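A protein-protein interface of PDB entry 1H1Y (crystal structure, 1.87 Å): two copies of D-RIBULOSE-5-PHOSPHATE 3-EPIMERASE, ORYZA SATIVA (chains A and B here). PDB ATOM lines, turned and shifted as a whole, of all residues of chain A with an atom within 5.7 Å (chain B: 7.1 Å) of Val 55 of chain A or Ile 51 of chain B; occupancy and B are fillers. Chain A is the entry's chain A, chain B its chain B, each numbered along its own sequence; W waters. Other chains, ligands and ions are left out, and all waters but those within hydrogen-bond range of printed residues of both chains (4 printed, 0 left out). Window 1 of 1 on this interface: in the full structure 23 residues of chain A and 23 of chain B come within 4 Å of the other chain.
The backbone NH of Leu 21 of chain A lies within hydrogen-bond range of the backbone carbonyl oxygen of Ala 19 of chain B, 3.4 Å away. N of Gly 52 of chain B sits at hydrogen-bond distance from O of Thr 50 of chain A (2.9 Å). O of Thr 50 of chain B sits at hydrogen-bond distance from N of Gly 52 of chain A (2.9 Å). The backbone NH (N) of Phe 18 of chain B lies within hydrogen-bond range of the side-chain hydroxyl (OG) of Ser 58 of chain A, 3.2 Å away.
The backbone carbonyl oxygen (O) of Pro 54 of chain A is in hydrogen-bond range of the side-chain hydroxyl (OG) of Ser 58 of chain A (3.4 Å). OD1 of Asp 17 of chain B is in hydrogen-bond range of N of Ala 19 of chain B, at 2.9 Å. The side-chain hydroxyl of Thr 50 of chain B is in hydrogen-bond range of the backbone carbonyl oxygen of Asp 39 of chain B (2.6 Å). The backbone NH (N) of Ile 40 of chain B is in hydrogen-bond range of the backbone carbonyl oxygen (O) of His 70 of chain B, 3.0 Å away. The backbone NH (N) of Met 41 of chain B lies within hydrogen-bond range of the side-chain hydroxyl (OG1) of Thr 50 of chain B.
Leu 49 of chain A touches Ile 51 of chain B. Gly 52 of chain B touches Leu 49 of chain A (N to CD2, 3.4 Å). Leu 49 of chain A touches Tyr 79 of chain B. Thr 50 of chain A touches Ile 51 of chain B. Ile 51 of chain A touches Thr 50 of chain B. CD2 of Leu 49 of chain B touches N of Gly 52 of chain A, 3.3 Å away. CA of Val 55 of chain A touches CB of Phe 18 of chain B (3.9 Å). Thr 50 of chain B touches Val 55 of chain A (O to CG2, 3.7 Å). Ile 51 of chain B touches Val 55 of chain A (CG2 to CG2, 3.7 Å). Ser 58 of chain A touches Asp 17 of chain B.
Of chain B, only Phe 18 (3.9 Å), Thr 50 (3.7 Å) and Ile 51 (3.7 Å) come within 4 Å of Val 55 of chain A. Ile 51 of chain B touches three residues of chain A. Of the printed residues of chain A, Val 55 of chain B touches Thr 50 and Ile 51. Of the printed residues of chain B, Ile 51 of chain A touches Leu 49, Thr 50 and Val 55. Of the printed residues of chain A, Phe 18 of chain B touches Pro 54, Val 55 and Ser 58. Of the printed residues of chain A, Gly 52 of chain B touches Leu 49 and Thr 50. Of the printed residues of chain B, Pro 54 of chain A touches Phe 18 (3.7 Å) and Leu 49 (3.2 Å). His 70 of chain B touches none of the printed residues of chain A. Gln 57 of chain A touches none of the printed residues of chain B.
Of the 24 printed residues of chain B, 13 touch a printed residue of chain A. Hydrophobic or aromatic side chains of chain B within 4 Å of the printed part of chain A: Phe 18, Ala 19, Ile 40, Leu 49, Ile 51, Pro 54, Val 55 and Tyr 79. Among the printed residues, no Asp or Glu carboxylate lies within 4 Å of a Lys or Arg side-chain nitrogen of the other chain.
Leu 49 of chain A touches Ile 51 of chain B, and with the chains exchanged Ile 51 of chain A touches Leu 49 of chain B. Leu 49 of chain A touches Gly 52 of chain B, and with the chains exchanged Gly 52 of chain A touches Leu 49 of chain B. Thr 50 of chain A touches Gly 52 of chain B, and with the chains exchanged Gly 52 of chain A touches Thr 50 of chain B. Positions printed for both chains: 21, 38, 49, 50, 51, 52, 53, 54, 55, 56 and 59. Of the 25 pairs that touch across the chains among the printed residues, 14 have their exchanged pair printed and touching as well.
Water W2 lies within hydrogen-bond range of the backbone carbonyl oxygen of Phe 18 of chain B, the backbone NH of Leu 21 of chain B, the backbone NH of Leu 21 of chain A and the backbone carbonyl oxygen of Ala 19 of chain B. Water W4 bridges the backbone NH of Ala 53 of chain A and the backbone carbonyl oxygen of Leu 49 of chain B. Water W1 lies within hydrogen-bond range of the backbone NH (N) of Ala 53 of chain B (2.7 Å) and the backbone carbonyl oxygen (O) of Leu 49 of chain A (2.9 Å).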
ATOM      1  N   LEU A  21      -8.922  26.176 -39.503  1.00  0.00           N
ATOM      2  CA  LEU A  21      -8.657  24.794 -39.902  1.00  0.00           C
ATOM      3  C   LEU A  21      -9.628  24.175 -40.905  1.00  0.00           C
ATOM      4  O   LEU A  21      -9.205  23.553 -41.884  1.00  0.00           O
ATOM      5  CB  LEU A  21      -8.587  23.891 -38.669  1.00  0.00           C
ATOM      6  CG  LEU A  21      -7.233  23.622 -38.015  1.00  0.00           C
ATOM      7  CD1 LEU A  21      -7.441  22.601 -36.888  1.00  0.00           C
ATOM      8  CD2 LEU A  21      -6.240  23.074 -39.056  1.00  0.00           C
ATOM      9  N   MET A  38      -1.870  15.443 -39.600  1.00  0.00           N
ATOM     10  CA  MET A  38      -2.062  16.111 -38.318  1.00  0.00           C
ATOM     11  C   MET A  38      -0.975  15.723 -37.328  1.00  0.00           C
ATOM     12  O   MET A  38      -0.916  14.585 -36.867  1.00  0.00           O
ATOM     13  CB  MET A  38      -3.432  15.742 -37.741  1.00  0.00           C
ATOM     14  CG  MET A  38      -4.559  15.758 -38.768  1.00  0.00           C
ATOM     15  SD  MET A  38      -4.829  17.359 -39.577  1.00  0.00           S
ATOM     16  CE  MET A  38      -5.477  18.312 -38.203  1.00  0.00           C
ATOM     17  N   LEU A  49       4.322  21.368 -28.400  1.00  0.00           N
ATOM     18  CA  LEU A  49       2.980  20.866 -28.112  1.00  0.00           C
ATOM     19  C   LEU A  49       2.111  21.499 -29.186  1.00  0.00           C
ATOM     20  O   LEU A  49       2.114  22.712 -29.339  1.00  0.00           O
ATOM     21  CB  LEU A  49       2.533  21.317 -26.712  1.00  0.00           C
ATOM     22  CG  LEU A  49       1.217  20.786 -26.118  1.00  0.00           C
ATOM     23  CD1 LEU A  49       1.078  21.285 -24.674  1.00  0.00           C
ATOM     24  CD2 LEU A  49       0.039  21.271 -26.936  1.00  0.00           C
ATOM     25  N   THR A  50       1.363  20.679 -29.919  1.00  0.00           N
ATOM     26  CA  THR A  50       0.557  21.185 -31.018  1.00  0.00           C
ATOM     27  C   THR A  50      -0.946  21.127 -30.841  1.00  0.00           C
ATOM     28  O   THR A  50      -1.563  22.121 -30.458  1.00  0.00           O
ATOM     29  CB  THR A  50       0.928  20.455 -32.331  1.00  0.00           C
ATOM     30  OG1 THR A  50       0.837  19.033 -32.136  1.00  0.00           O
ATOM     31  CG2 THR A  50       2.359  20.799 -32.739  1.00  0.00           C
ATOM     32  N   ILE A  51      -1.528  19.971 -31.152  1.00  0.00           N
ATOM     33  CA  ILE A  51      -2.968  19.766 -31.037  1.00  0.00           C
ATOM     34  C   ILE A  51      -3.235  18.332 -30.607  1.00  0.00           C
ATOM     35  O   ILE A  51      -2.396  17.442 -30.797  1.00  0.00           O
ATOM     36  CB  ILE A  51      -3.699  20.003 -32.394  1.00  0.00           C
ATOM     37  CG1 ILE A  51      -3.044  19.159 -33.490  1.00  0.00           C
ATOM     38  CG2 ILE A  51      -3.628  21.483 -32.788  1.00  0.00           C
ATOM     39  CD1 ILE A  51      -3.867  19.072 -34.770  1.00  0.00           C
ATOM     40  N   GLY A  52      -4.410  18.110 -30.032  1.00  0.00           N
ATOM     41  CA  GLY A  52      -4.768  16.776 -29.597  1.00  0.00           C
ATOM     42  C   GLY A  52      -6.097  16.339 -30.186  1.00  0.00           C
ATOM     43  O   GLY A  52      -6.623  16.968 -31.111  1.00  0.00           O
ATOM     44  N   ALA A  53      -6.652  15.268 -29.624  1.00  0.00           N
ATOM     45  CA  ALA A  53      -7.916  14.706 -30.101  1.00  0.00           C
ATOM     46  C   ALA A  53      -9.095  15.685 -30.144  1.00  0.00           C
ATOM     47  O   ALA A  53      -9.962  15.581 -31.018  1.00  0.00           O
ATOM     48  CB  ALA A  53      -8.283  13.457 -29.262  1.00  0.00           C
ATOM     49  N   PRO A  54      -9.151  16.646 -29.212  1.00  0.00           N
ATOM     50  CA  PRO A  54     -10.287  17.572 -29.274  1.00  0.00           C
ATOM     51  C   PRO A  54     -10.310  18.348 -30.593  1.00  0.00           C
ATOM     52  O   PRO A  54     -11.374  18.645 -31.134  1.00  0.00           O
ATOM     53  CB  PRO A  54     -10.052  18.480 -28.073  1.00  0.00           C
ATOM     54  CG  PRO A  54      -9.408  17.543 -27.079  1.00  0.00           C
ATOM     55  CD  PRO A  54      -8.394  16.831 -27.958  1.00  0.00           C
ATOM     56  N   VAL A  55      -9.128  18.669 -31.105  1.00  0.00           N
ATOM     57  CA  VAL A  55      -9.023  19.408 -32.364  1.00  0.00           C
ATOM     58  C   VAL A  55      -9.425  18.519 -33.536  1.00  0.00           C
ATOM     59  O   VAL A  55     -10.142  18.955 -34.439  1.00  0.00           O
ATOM     60  CB  VAL A  55      -7.587  19.935 -32.569  1.00  0.00           C
ATOM     61  CG1 VAL A  55      -7.459  20.625 -33.929  1.00  0.00           C
ATOM     62  CG2 VAL A  55      -7.254  20.925 -31.448  1.00  0.00           C
ATOM     63  N   ILE A  56      -8.974  17.268 -33.506  1.00  0.00           N
ATOM     64  CA  ILE A  56      -9.302  16.309 -34.559  1.00  0.00           C
ATOM     65  C   ILE A  56     -10.824  16.121 -34.586  1.00  0.00           C
ATOM     66  O   ILE A  56     -11.445  16.078 -35.651  1.00  0.00           O
ATOM     67  CB  ILE A  56      -8.642  14.933 -34.291  1.00  0.00           C
ATOM     68  CG1 ILE A  56      -7.113  15.072 -34.202  1.00  0.00           C
ATOM     69  CG2 ILE A  56      -9.041  13.940 -35.389  1.00  0.00           C
ATOM     70  CD1 ILE A  56      -6.464  15.676 -35.445  1.00  0.00           C
ATOM     71  N   GLN A  57     -11.428  16.003 -33.407  1.00  0.00           N
ATOM     72  CA  GLN A  57     -12.874  15.810 -33.330  1.00  0.00           C
ATOM     73  C   GLN A  57     -13.633  16.971 -33.974  1.00  0.00           C
ATOM     74  O   GLN A  57     -14.571  16.762 -34.751  1.00  0.00           O
ATOM     75  CB  GLN A  57     -13.288  15.642 -31.869  1.00  0.00           C
ATOM     76  CG  GLN A  57     -14.699  15.134 -31.677  1.00  0.00           C
ATOM     77  CD  GLN A  57     -14.888  14.494 -30.313  1.00  0.00           C
ATOM     78  OE1 GLN A  57     -14.290  13.453 -30.008  1.00  0.00           O
ATOM     79  NE2 GLN A  57     -15.718  15.109 -29.486  1.00  0.00           N
ATOM     80  N   SER A  58     -13.247  18.202 -33.653  1.00  0.00           N
ATOM     81  CA  SER A  58     -13.916  19.350 -34.248  1.00  0.00           C
ATOM     82  C   SER A  58     -13.710  19.348 -35.766  1.00  0.00           C
ATOM     83  O   SER A  58     -14.647  19.596 -36.517  1.00  0.00           O
ATOM     84  CB  SER A  58     -13.378  20.663 -33.661  1.00  0.00           C
ATOM     85  OG  SER A  58     -13.750  20.821 -32.296  1.00  0.00           O
ATOM     86  N   LEU A  59     -12.496  19.053 -36.221  1.00  0.00           N
ATOM     87  CA  LEU A  59     -12.240  19.052 -37.660  1.00  0.00           C
ATOM     88  C   LEU A  59     -13.066  18.006 -38.408  1.00  0.00           C
ATOM     89  O   LEU A  59     -13.601  18.291 -39.488  1.00  0.00           O
ATOM     90  CB  LEU A  59     -10.757  18.837 -37.954  1.00  0.00           C
ATOM     91  CG  LEU A  59     -10.390  18.786 -39.445  1.00  0.00           C
ATOM     92  CD1 LEU A  59     -10.820  20.071 -40.157  1.00  0.00           C
ATOM     93  CD2 LEU A  59      -8.895  18.582 -39.578  1.00  0.00           C
ATOM     94  N   ARG A  60     -13.180  16.810 -37.832  1.00  0.00           N
ATOM     95  CA  ARG A  60     -13.943  15.731 -38.462  1.00  0.00           C
ATOM     96  C   ARG A  60     -15.405  16.121 -38.706  1.00  0.00           C
ATOM     97  O   ARG A  60     -16.042  15.618 -39.632  1.00  0.00           O
ATOM     98  CB  ARG A  60     -13.868  14.453 -37.609  1.00  0.00           C
ATOM     99  CG  ARG A  60     -14.743  13.294 -38.119  1.00  0.00           C
ATOM    100  CD  ARG A  60     -14.438  12.945 -39.579  1.00  0.00           C
ATOM    101  NE  ARG A  60     -13.204  12.179 -39.764  1.00  0.00           N
ATOM    102  CZ  ARG A  60     -12.437  12.259 -40.854  1.00  0.00           C
ATOM    103  NH1 ARG A  60     -12.775  13.080 -41.836  1.00  0.00           N
ATOM    104  NH2 ARG A  60     -11.354  11.496 -40.983  1.00  0.00           N
ATOM    105  N   MET B  13     -12.316  28.226 -24.624  1.00  0.00           N
ATOM    106  CA  MET B  13     -12.288  27.757 -25.999  1.00  0.00           C
ATOM    107  C   MET B  13     -12.209  26.248 -26.134  1.00  0.00           C
ATOM    108  O   MET B  13     -12.398  25.711 -27.219  1.00  0.00           O
ATOM    109  CB  MET B  13     -11.158  28.463 -26.763  1.00  0.00           C
ATOM    110  CG  MET B  13     -11.282  29.999 -26.744  1.00  0.00           C
ATOM    111  SD  MET B  13     -12.922  30.682 -27.185  1.00  0.00           S
ATOM    112  CE  MET B  13     -12.873  30.497 -28.991  1.00  0.00           C
ATOM    113  N   LEU B  14     -11.954  25.563 -25.023  1.00  0.00           N
ATOM    114  CA  LEU B  14     -11.906  24.101 -25.016  1.00  0.00           C
ATOM    115  C   LEU B  14     -13.286  23.547 -25.407  1.00  0.00           C
ATOM    116  O   LEU B  14     -13.408  22.398 -25.843  1.00  0.00           O
ATOM    117  CB  LEU B  14     -11.531  23.599 -23.615  1.00  0.00           C
ATOM    118  CG  LEU B  14     -11.588  22.091 -23.327  1.00  0.00           C
ATOM    119  CD1 LEU B  14     -10.593  21.349 -24.210  1.00  0.00           C
ATOM    120  CD2 LEU B  14     -11.283  21.843 -21.852  1.00  0.00           C
ATOM    121  N   ASP B  17     -15.642  25.310 -31.296  1.00  0.00           N
ATOM    122  CA  ASP B  17     -15.374  24.569 -32.517  1.00  0.00           C
ATOM    123  C   ASP B  17     -13.906  24.834 -32.845  1.00  0.00           C
ATOM    124  O   ASP B  17     -13.576  25.871 -33.426  1.00  0.00           O
ATOM    125  CB  ASP B  17     -16.262  25.096 -33.643  1.00  0.00           C
ATOM    126  CG  ASP B  17     -16.001  24.401 -34.966  1.00  0.00           C
ATOM    127  OD1 ASP B  17     -15.000  23.657 -35.065  1.00  0.00           O
ATOM    128  OD2 ASP B  17     -16.793  24.607 -35.908  1.00  0.00           O
ATOM    129  N   PHE B  18     -13.027  23.911 -32.459  1.00  0.00           N
ATOM    130  CA  PHE B  18     -11.597  24.067 -32.705  1.00  0.00           C
ATOM    131  C   PHE B  18     -11.231  24.229 -34.180  1.00  0.00           C
ATOM    132  O   PHE B  18     -10.112  24.632 -34.492  1.00  0.00           O
ATOM    133  CB  PHE B  18     -10.811  22.874 -32.140  1.00  0.00           C
ATOM    134  CG  PHE B  18     -10.529  22.965 -30.663  1.00  0.00           C
ATOM    135  CD1 PHE B  18     -11.116  22.068 -29.769  1.00  0.00           C
ATOM    136  CD2 PHE B  18      -9.657  23.928 -30.170  1.00  0.00           C
ATOM    137  CE1 PHE B  18     -10.831  22.129 -28.403  1.00  0.00           C
ATOM    138  CE2 PHE B  18      -9.365  23.999 -28.808  1.00  0.00           C
ATOM    139  CZ  PHE B  18      -9.951  23.098 -27.923  1.00  0.00           C
ATOM    140  N   ALA B  19     -12.147  23.892 -35.083  1.00  0.00           N
ATOM    141  CA  ALA B  19     -11.872  24.011 -36.518  1.00  0.00           C
ATOM    142  C   ALA B  19     -12.253  25.375 -37.097  1.00  0.00           C
ATOM    143  O   ALA B  19     -12.045  25.637 -38.284  1.00  0.00           O
ATOM    144  CB  ALA B  19     -12.588  22.903 -37.277  1.00  0.00           C
ATOM    145  N   LEU B  21     -11.691  28.409 -34.979  1.00  0.00           N
ATOM    146  CA  LEU B  21     -11.280  29.208 -33.832  1.00  0.00           C
ATOM    147  C   LEU B  21     -11.367  30.711 -34.005  1.00  0.00           C
ATOM    148  O   LEU B  21     -11.789  31.406 -33.085  1.00  0.00           O
ATOM    149  CB  LEU B  21      -9.849  28.857 -33.400  1.00  0.00           C
ATOM    150  CG  LEU B  21      -9.642  27.707 -32.404  1.00  0.00           C
ATOM    151  CD1 LEU B  21      -8.147  27.577 -32.121  1.00  0.00           C
ATOM    152  CD2 LEU B  21     -10.410  27.963 -31.103  1.00  0.00           C
ATOM    153  N   HIS B  37     -10.340  32.271 -22.775  1.00  0.00           N
ATOM    154  CA  HIS B  37      -9.548  31.358 -21.959  1.00  0.00           C
ATOM    155  C   HIS B  37      -9.029  30.178 -22.780  1.00  0.00           C
ATOM    156  O   HIS B  37      -9.807  29.369 -23.292  1.00  0.00           O
ATOM    157  CB  HIS B  37     -10.381  30.856 -20.777  1.00  0.00           C
ATOM    158  CG  HIS B  37      -9.570  30.164 -19.726  1.00  0.00           C
ATOM    159  ND1 HIS B  37      -8.782  30.846 -18.824  1.00  0.00           N
ATOM    160  CD2 HIS B  37      -9.393  28.850 -19.461  1.00  0.00           C
ATOM    161  CE1 HIS B  37      -8.153  29.982 -18.048  1.00  0.00           C
ATOM    162  NE2 HIS B  37      -8.506  28.764 -18.415  1.00  0.00           N
ATOM    163  N   MET B  38      -7.705  30.076 -22.895  1.00  0.00           N
ATOM    164  CA  MET B  38      -7.088  29.017 -23.691  1.00  0.00           C
ATOM    165  C   MET B  38      -6.460  27.938 -22.812  1.00  0.00           C
ATOM    166  O   MET B  38      -5.450  28.176 -22.159  1.00  0.00           O
ATOM    167  CB  MET B  38      -6.010  29.620 -24.598  1.00  0.00           C
ATOM    168  CG  MET B  38      -6.423  30.904 -25.300  1.00  0.00           C
ATOM    169  SD  MET B  38      -7.959  30.740 -26.243  1.00  0.00           S
ATOM    170  CE  MET B  38      -7.370  29.741 -27.639  1.00  0.00           C
ATOM    171  N   ASP B  39      -7.063  26.754 -22.804  1.00  0.00           N
ATOM    172  CA  ASP B  39      -6.569  25.639 -22.007  1.00  0.00           C
ATOM    173  C   ASP B  39      -5.493  24.857 -22.740  1.00  0.00           C
ATOM    174  O   ASP B  39      -5.777  24.207 -23.731  1.00  0.00           O
ATOM    175  CB  ASP B  39      -7.720  24.711 -21.657  1.00  0.00           C
ATOM    176  CG  ASP B  39      -8.627  25.303 -20.618  1.00  0.00           C
ATOM    177  OD1 ASP B  39      -8.134  25.486 -19.489  1.00  0.00           O
ATOM    178  OD2 ASP B  39      -9.803  25.597 -20.930  1.00  0.00           O
ATOM    179  N   ILE B  40      -4.264  24.940 -22.240  1.00  0.00           N
ATOM    180  CA  ILE B  40      -3.120  24.249 -22.822  1.00  0.00           C
ATOM    181  C   ILE B  40      -2.783  23.065 -21.917  1.00  0.00           C
ATOM    182  O   ILE B  40      -2.316  23.244 -20.792  1.00  0.00           O
ATOM    183  CB  ILE B  40      -1.921  25.210 -22.928  1.00  0.00           C
ATOM    184  CG1 ILE B  40      -2.310  26.397 -23.820  1.00  0.00           C
ATOM    185  CG2 ILE B  40      -0.693  24.472 -23.462  1.00  0.00           C
ATOM    186  CD1 ILE B  40      -1.323  27.540 -23.808  1.00  0.00           C
ATOM    187  N   MET B  41      -3.036  21.859 -22.420  1.00  0.00           N
ATOM    188  CA  MET B  41      -2.822  20.615 -21.675  1.00  0.00           C
ATOM    189  C   MET B  41      -1.850  19.724 -22.447  1.00  0.00           C
ATOM    190  O   MET B  41      -2.017  19.554 -23.653  1.00  0.00           O
ATOM    191  CB  MET B  41      -4.164  19.894 -21.524  1.00  0.00           C
ATOM    192  CG  MET B  41      -5.263  20.743 -20.888  1.00  0.00           C
ATOM    193  SD  MET B  41      -6.774  19.769 -20.681  1.00  0.00           S
ATOM    194  CE  MET B  41      -8.003  21.069 -20.291  1.00  0.00           C
ATOM    195  N   ASP B  42      -0.862  19.138 -21.758  1.00  0.00           N
ATOM    196  CA  ASP B  42       0.146  18.315 -22.420  1.00  0.00           C
ATOM    197  C   ASP B  42       0.020  16.799 -22.264  1.00  0.00           C
ATOM    198  O   ASP B  42       0.969  16.079 -22.560  1.00  0.00           O
ATOM    199  CB  ASP B  42       1.561  18.741 -21.968  1.00  0.00           C
ATOM    200  CG  ASP B  42       1.851  18.396 -20.500  1.00  0.00           C
ATOM    201  OD1 ASP B  42       0.954  17.865 -19.812  1.00  0.00           O
ATOM    202  OD2 ASP B  42       2.984  18.661 -20.036  1.00  0.00           O
ATOM    203  N   LEU B  49      -4.825  16.259 -23.984  1.00  0.00           N
ATOM    204  CA  LEU B  49      -3.895  17.064 -24.771  1.00  0.00           C
ATOM    205  C   LEU B  49      -4.802  17.941 -25.632  1.00  0.00           C
ATOM    206  O   LEU B  49      -5.617  17.423 -26.382  1.00  0.00           O
ATOM    207  CB  LEU B  49      -3.031  16.147 -25.643  1.00  0.00           C
ATOM    208  CG  LEU B  49      -1.880  16.789 -26.436  1.00  0.00           C
ATOM    209  CD1 LEU B  49      -1.171  15.698 -27.232  1.00  0.00           C
ATOM    210  CD2 LEU B  49      -2.395  17.854 -27.382  1.00  0.00           C
ATOM    211  N   THR B  50      -4.641  19.260 -25.540  1.00  0.00           N
ATOM    212  CA  THR B  50      -5.512  20.177 -26.268  1.00  0.00           C
ATOM    213  C   THR B  50      -4.878  20.970 -27.406  1.00  0.00           C
ATOM    214  O   THR B  50      -4.927  20.553 -28.559  1.00  0.00           O
ATOM    215  CB  THR B  50      -6.165  21.165 -25.282  1.00  0.00           C
ATOM    216  OG1 THR B  50      -5.140  21.818 -24.515  1.00  0.00           O
ATOM    217  CG2 THR B  50      -7.106  20.411 -24.321  1.00  0.00           C
ATOM    218  N   ILE B  51      -4.310  22.131 -27.079  1.00  0.00           N
ATOM    219  CA  ILE B  51      -3.672  22.991 -28.077  1.00  0.00           C
ATOM    220  C   ILE B  51      -2.435  23.622 -27.454  1.00  0.00           C
ATOM    221  O   ILE B  51      -2.354  23.740 -26.228  1.00  0.00           O
ATOM    222  CB  ILE B  51      -4.616  24.126 -28.540  1.00  0.00           C
ATOM    223  CG1 ILE B  51      -5.160  24.887 -27.324  1.00  0.00           C
ATOM    224  CG2 ILE B  51      -5.774  23.536 -29.349  1.00  0.00           C
ATOM    225  CD1 ILE B  51      -5.858  26.203 -27.662  1.00  0.00           C
ATOM    226  N   GLY B  52      -1.483  24.025 -28.294  1.00  0.00           N
ATOM    227  CA  GLY B  52      -0.268  24.641 -27.784  1.00  0.00           C
ATOM    228  C   GLY B  52       0.016  25.996 -28.411  1.00  0.00           C
ATOM    229  O   GLY B  52      -0.857  26.590 -29.056  1.00  0.00           O
ATOM    230  N   ALA B  53       1.250  26.472 -28.261  1.00  0.00           N
ATOM    231  CA  ALA B  53       1.620  27.783 -28.802  1.00  0.00           C
ATOM    232  C   ALA B  53       1.361  27.967 -30.301  1.00  0.00           C
ATOM    233  O   ALA B  53       0.989  29.058 -30.732  1.00  0.00           O
ATOM    234  CB  ALA B  53       3.079  28.091 -28.470  1.00  0.00           C
ATOM    235  N   PRO B  54       1.554  26.918 -31.116  1.00  0.00           N
ATOM    236  CA  PRO B  54       1.296  27.112 -32.550  1.00  0.00           C
ATOM    237  C   PRO B  54      -0.151  27.540 -32.818  1.00  0.00           C
ATOM    238  O   PRO B  54      -0.426  28.321 -33.737  1.00  0.00           O
ATOM    239  CB  PRO B  54       1.615  25.738 -33.150  1.00  0.00           C
ATOM    240  CG  PRO B  54       2.681  25.200 -32.208  1.00  0.00           C
ATOM    241  CD  PRO B  54       2.125  25.583 -30.856  1.00  0.00           C
ATOM    242  N   VAL B  55      -1.078  27.040 -32.011  1.00  0.00           N
ATOM    243  CA  VAL B  55      -2.490  27.391 -32.194  1.00  0.00           C
ATOM    244  C   VAL B  55      -2.723  28.826 -31.725  1.00  0.00           C
ATOM    245  O   VAL B  55      -3.419  29.599 -32.381  1.00  0.00           O
ATOM    246  CB  VAL B  55      -3.407  26.421 -31.421  1.00  0.00           C
ATOM    247  CG1 VAL B  55      -4.865  26.857 -31.540  1.00  0.00           C
ATOM    248  CG2 VAL B  55      -3.232  25.005 -31.971  1.00  0.00           C
ATOM    249  N   ILE B  56      -2.113  29.182 -30.599  1.00  0.00           N
ATOM    250  CA  ILE B  56      -2.234  30.535 -30.050  1.00  0.00           C
ATOM    251  C   ILE B  56      -1.678  31.541 -31.057  1.00  0.00           C
ATOM    252  O   ILE B  56      -2.256  32.608 -31.271  1.00  0.00           O
ATOM    253  CB  ILE B  56      -1.437  30.691 -28.730  1.00  0.00           C
ATOM    254  CG1 ILE B  56      -1.961  29.709 -27.678  1.00  0.00           C
ATOM    255  CG2 ILE B  56      -1.549  32.135 -28.200  1.00  0.00           C
ATOM    256  CD1 ILE B  56      -3.463  29.838 -27.398  1.00  0.00           C
ATOM    257  N   LEU B  59      -4.136  32.053 -33.857  1.00  0.00           N
ATOM    258  CA  LEU B  59      -5.302  32.804 -33.391  1.00  0.00           C
ATOM    259  C   LEU B  59      -4.996  34.295 -33.226  1.00  0.00           C
ATOM    260  O   LEU B  59      -5.806  35.142 -33.611  1.00  0.00           O
ATOM    261  CB  LEU B  59      -5.827  32.238 -32.068  1.00  0.00           C
ATOM    262  CG  LEU B  59      -7.026  32.991 -31.480  1.00  0.00           C
ATOM    263  CD1 LEU B  59      -8.148  33.085 -32.521  1.00  0.00           C
ATOM    264  CD2 LEU B  59      -7.516  32.285 -30.219  1.00  0.00           C
ATOM    265  N   HIS B  70      -3.921  29.185 -19.874  1.00  0.00           N
ATOM    266  CA  HIS B  70      -3.787  28.390 -18.669  1.00  0.00           C
ATOM    267  C   HIS B  70      -2.928  27.162 -19.004  1.00  0.00           C
ATOM    268  O   HIS B  70      -3.331  26.290 -19.779  1.00  0.00           O
ATOM    269  CB  HIS B  70      -5.189  27.992 -18.194  1.00  0.00           C
ATOM    270  CG  HIS B  70      -5.199  27.121 -16.978  1.00  0.00           C
ATOM    271  ND1 HIS B  70      -6.336  26.478 -16.538  1.00  0.00           N
ATOM    272  CD2 HIS B  70      -4.211  26.762 -16.130  1.00  0.00           C
ATOM    273  CE1 HIS B  70      -6.045  25.755 -15.475  1.00  0.00           C
ATOM    274  NE2 HIS B  70      -4.764  25.908 -15.206  1.00  0.00           N
ATOM    275  N   VAL B  73       0.515  22.000 -17.887  1.00  0.00           N
ATOM    276  CA  VAL B  73       1.664  21.263 -18.393  1.00  0.00           C
ATOM    277  C   VAL B  73       2.627  21.054 -17.239  1.00  0.00           C
ATOM    278  O   VAL B  73       2.588  21.781 -16.246  1.00  0.00           O
ATOM    279  CB  VAL B  73       2.404  22.065 -19.498  1.00  0.00           C
ATOM    280  CG1 VAL B  73       1.438  22.410 -20.625  1.00  0.00           C
ATOM    281  CG2 VAL B  73       3.001  23.351 -18.906  1.00  0.00           C
ATOM    282  N   TYR B  79       7.403  27.056 -21.847  1.00  0.00           N
ATOM    283  CA  TYR B  79       6.363  27.641 -22.690  1.00  0.00           C
ATOM    284  C   TYR B  79       6.364  29.165 -22.680  1.00  0.00           C
ATOM    285  O   TYR B  79       5.673  29.794 -23.481  1.00  0.00           O
ATOM    286  CB  TYR B  79       4.975  27.160 -22.265  1.00  0.00           C
ATOM    287  CG  TYR B  79       4.739  25.703 -22.591  1.00  0.00           C
ATOM    288  CD1 TYR B  79       5.247  24.696 -21.768  1.00  0.00           C
ATOM    289  CD2 TYR B  79       4.068  25.332 -23.757  1.00  0.00           C
ATOM    290  CE1 TYR B  79       5.095  23.347 -22.100  1.00  0.00           C
ATOM    291  CE2 TYR B  79       3.914  23.983 -24.103  1.00  0.00           C
ATOM    292  CZ  TYR B  79       4.434  23.004 -23.271  1.00  0.00           C
ATOM    293  OH  TYR B  79       4.323  21.687 -23.628  1.00  0.00           O
HETATM  294  O   HOH W   1       3.110  24.673 -27.449  1.00  0.00           O
HETATM  295  O   HOH W   2      -9.392  26.541 -36.219  1.00  0.00           O
HETATM  296  O   HOH W   3     -16.535  21.240 -35.365  1.00  0.00           O
HETATM  297  O   HOH W   4      -5.711  14.560 -27.211  1.00  0.00           O
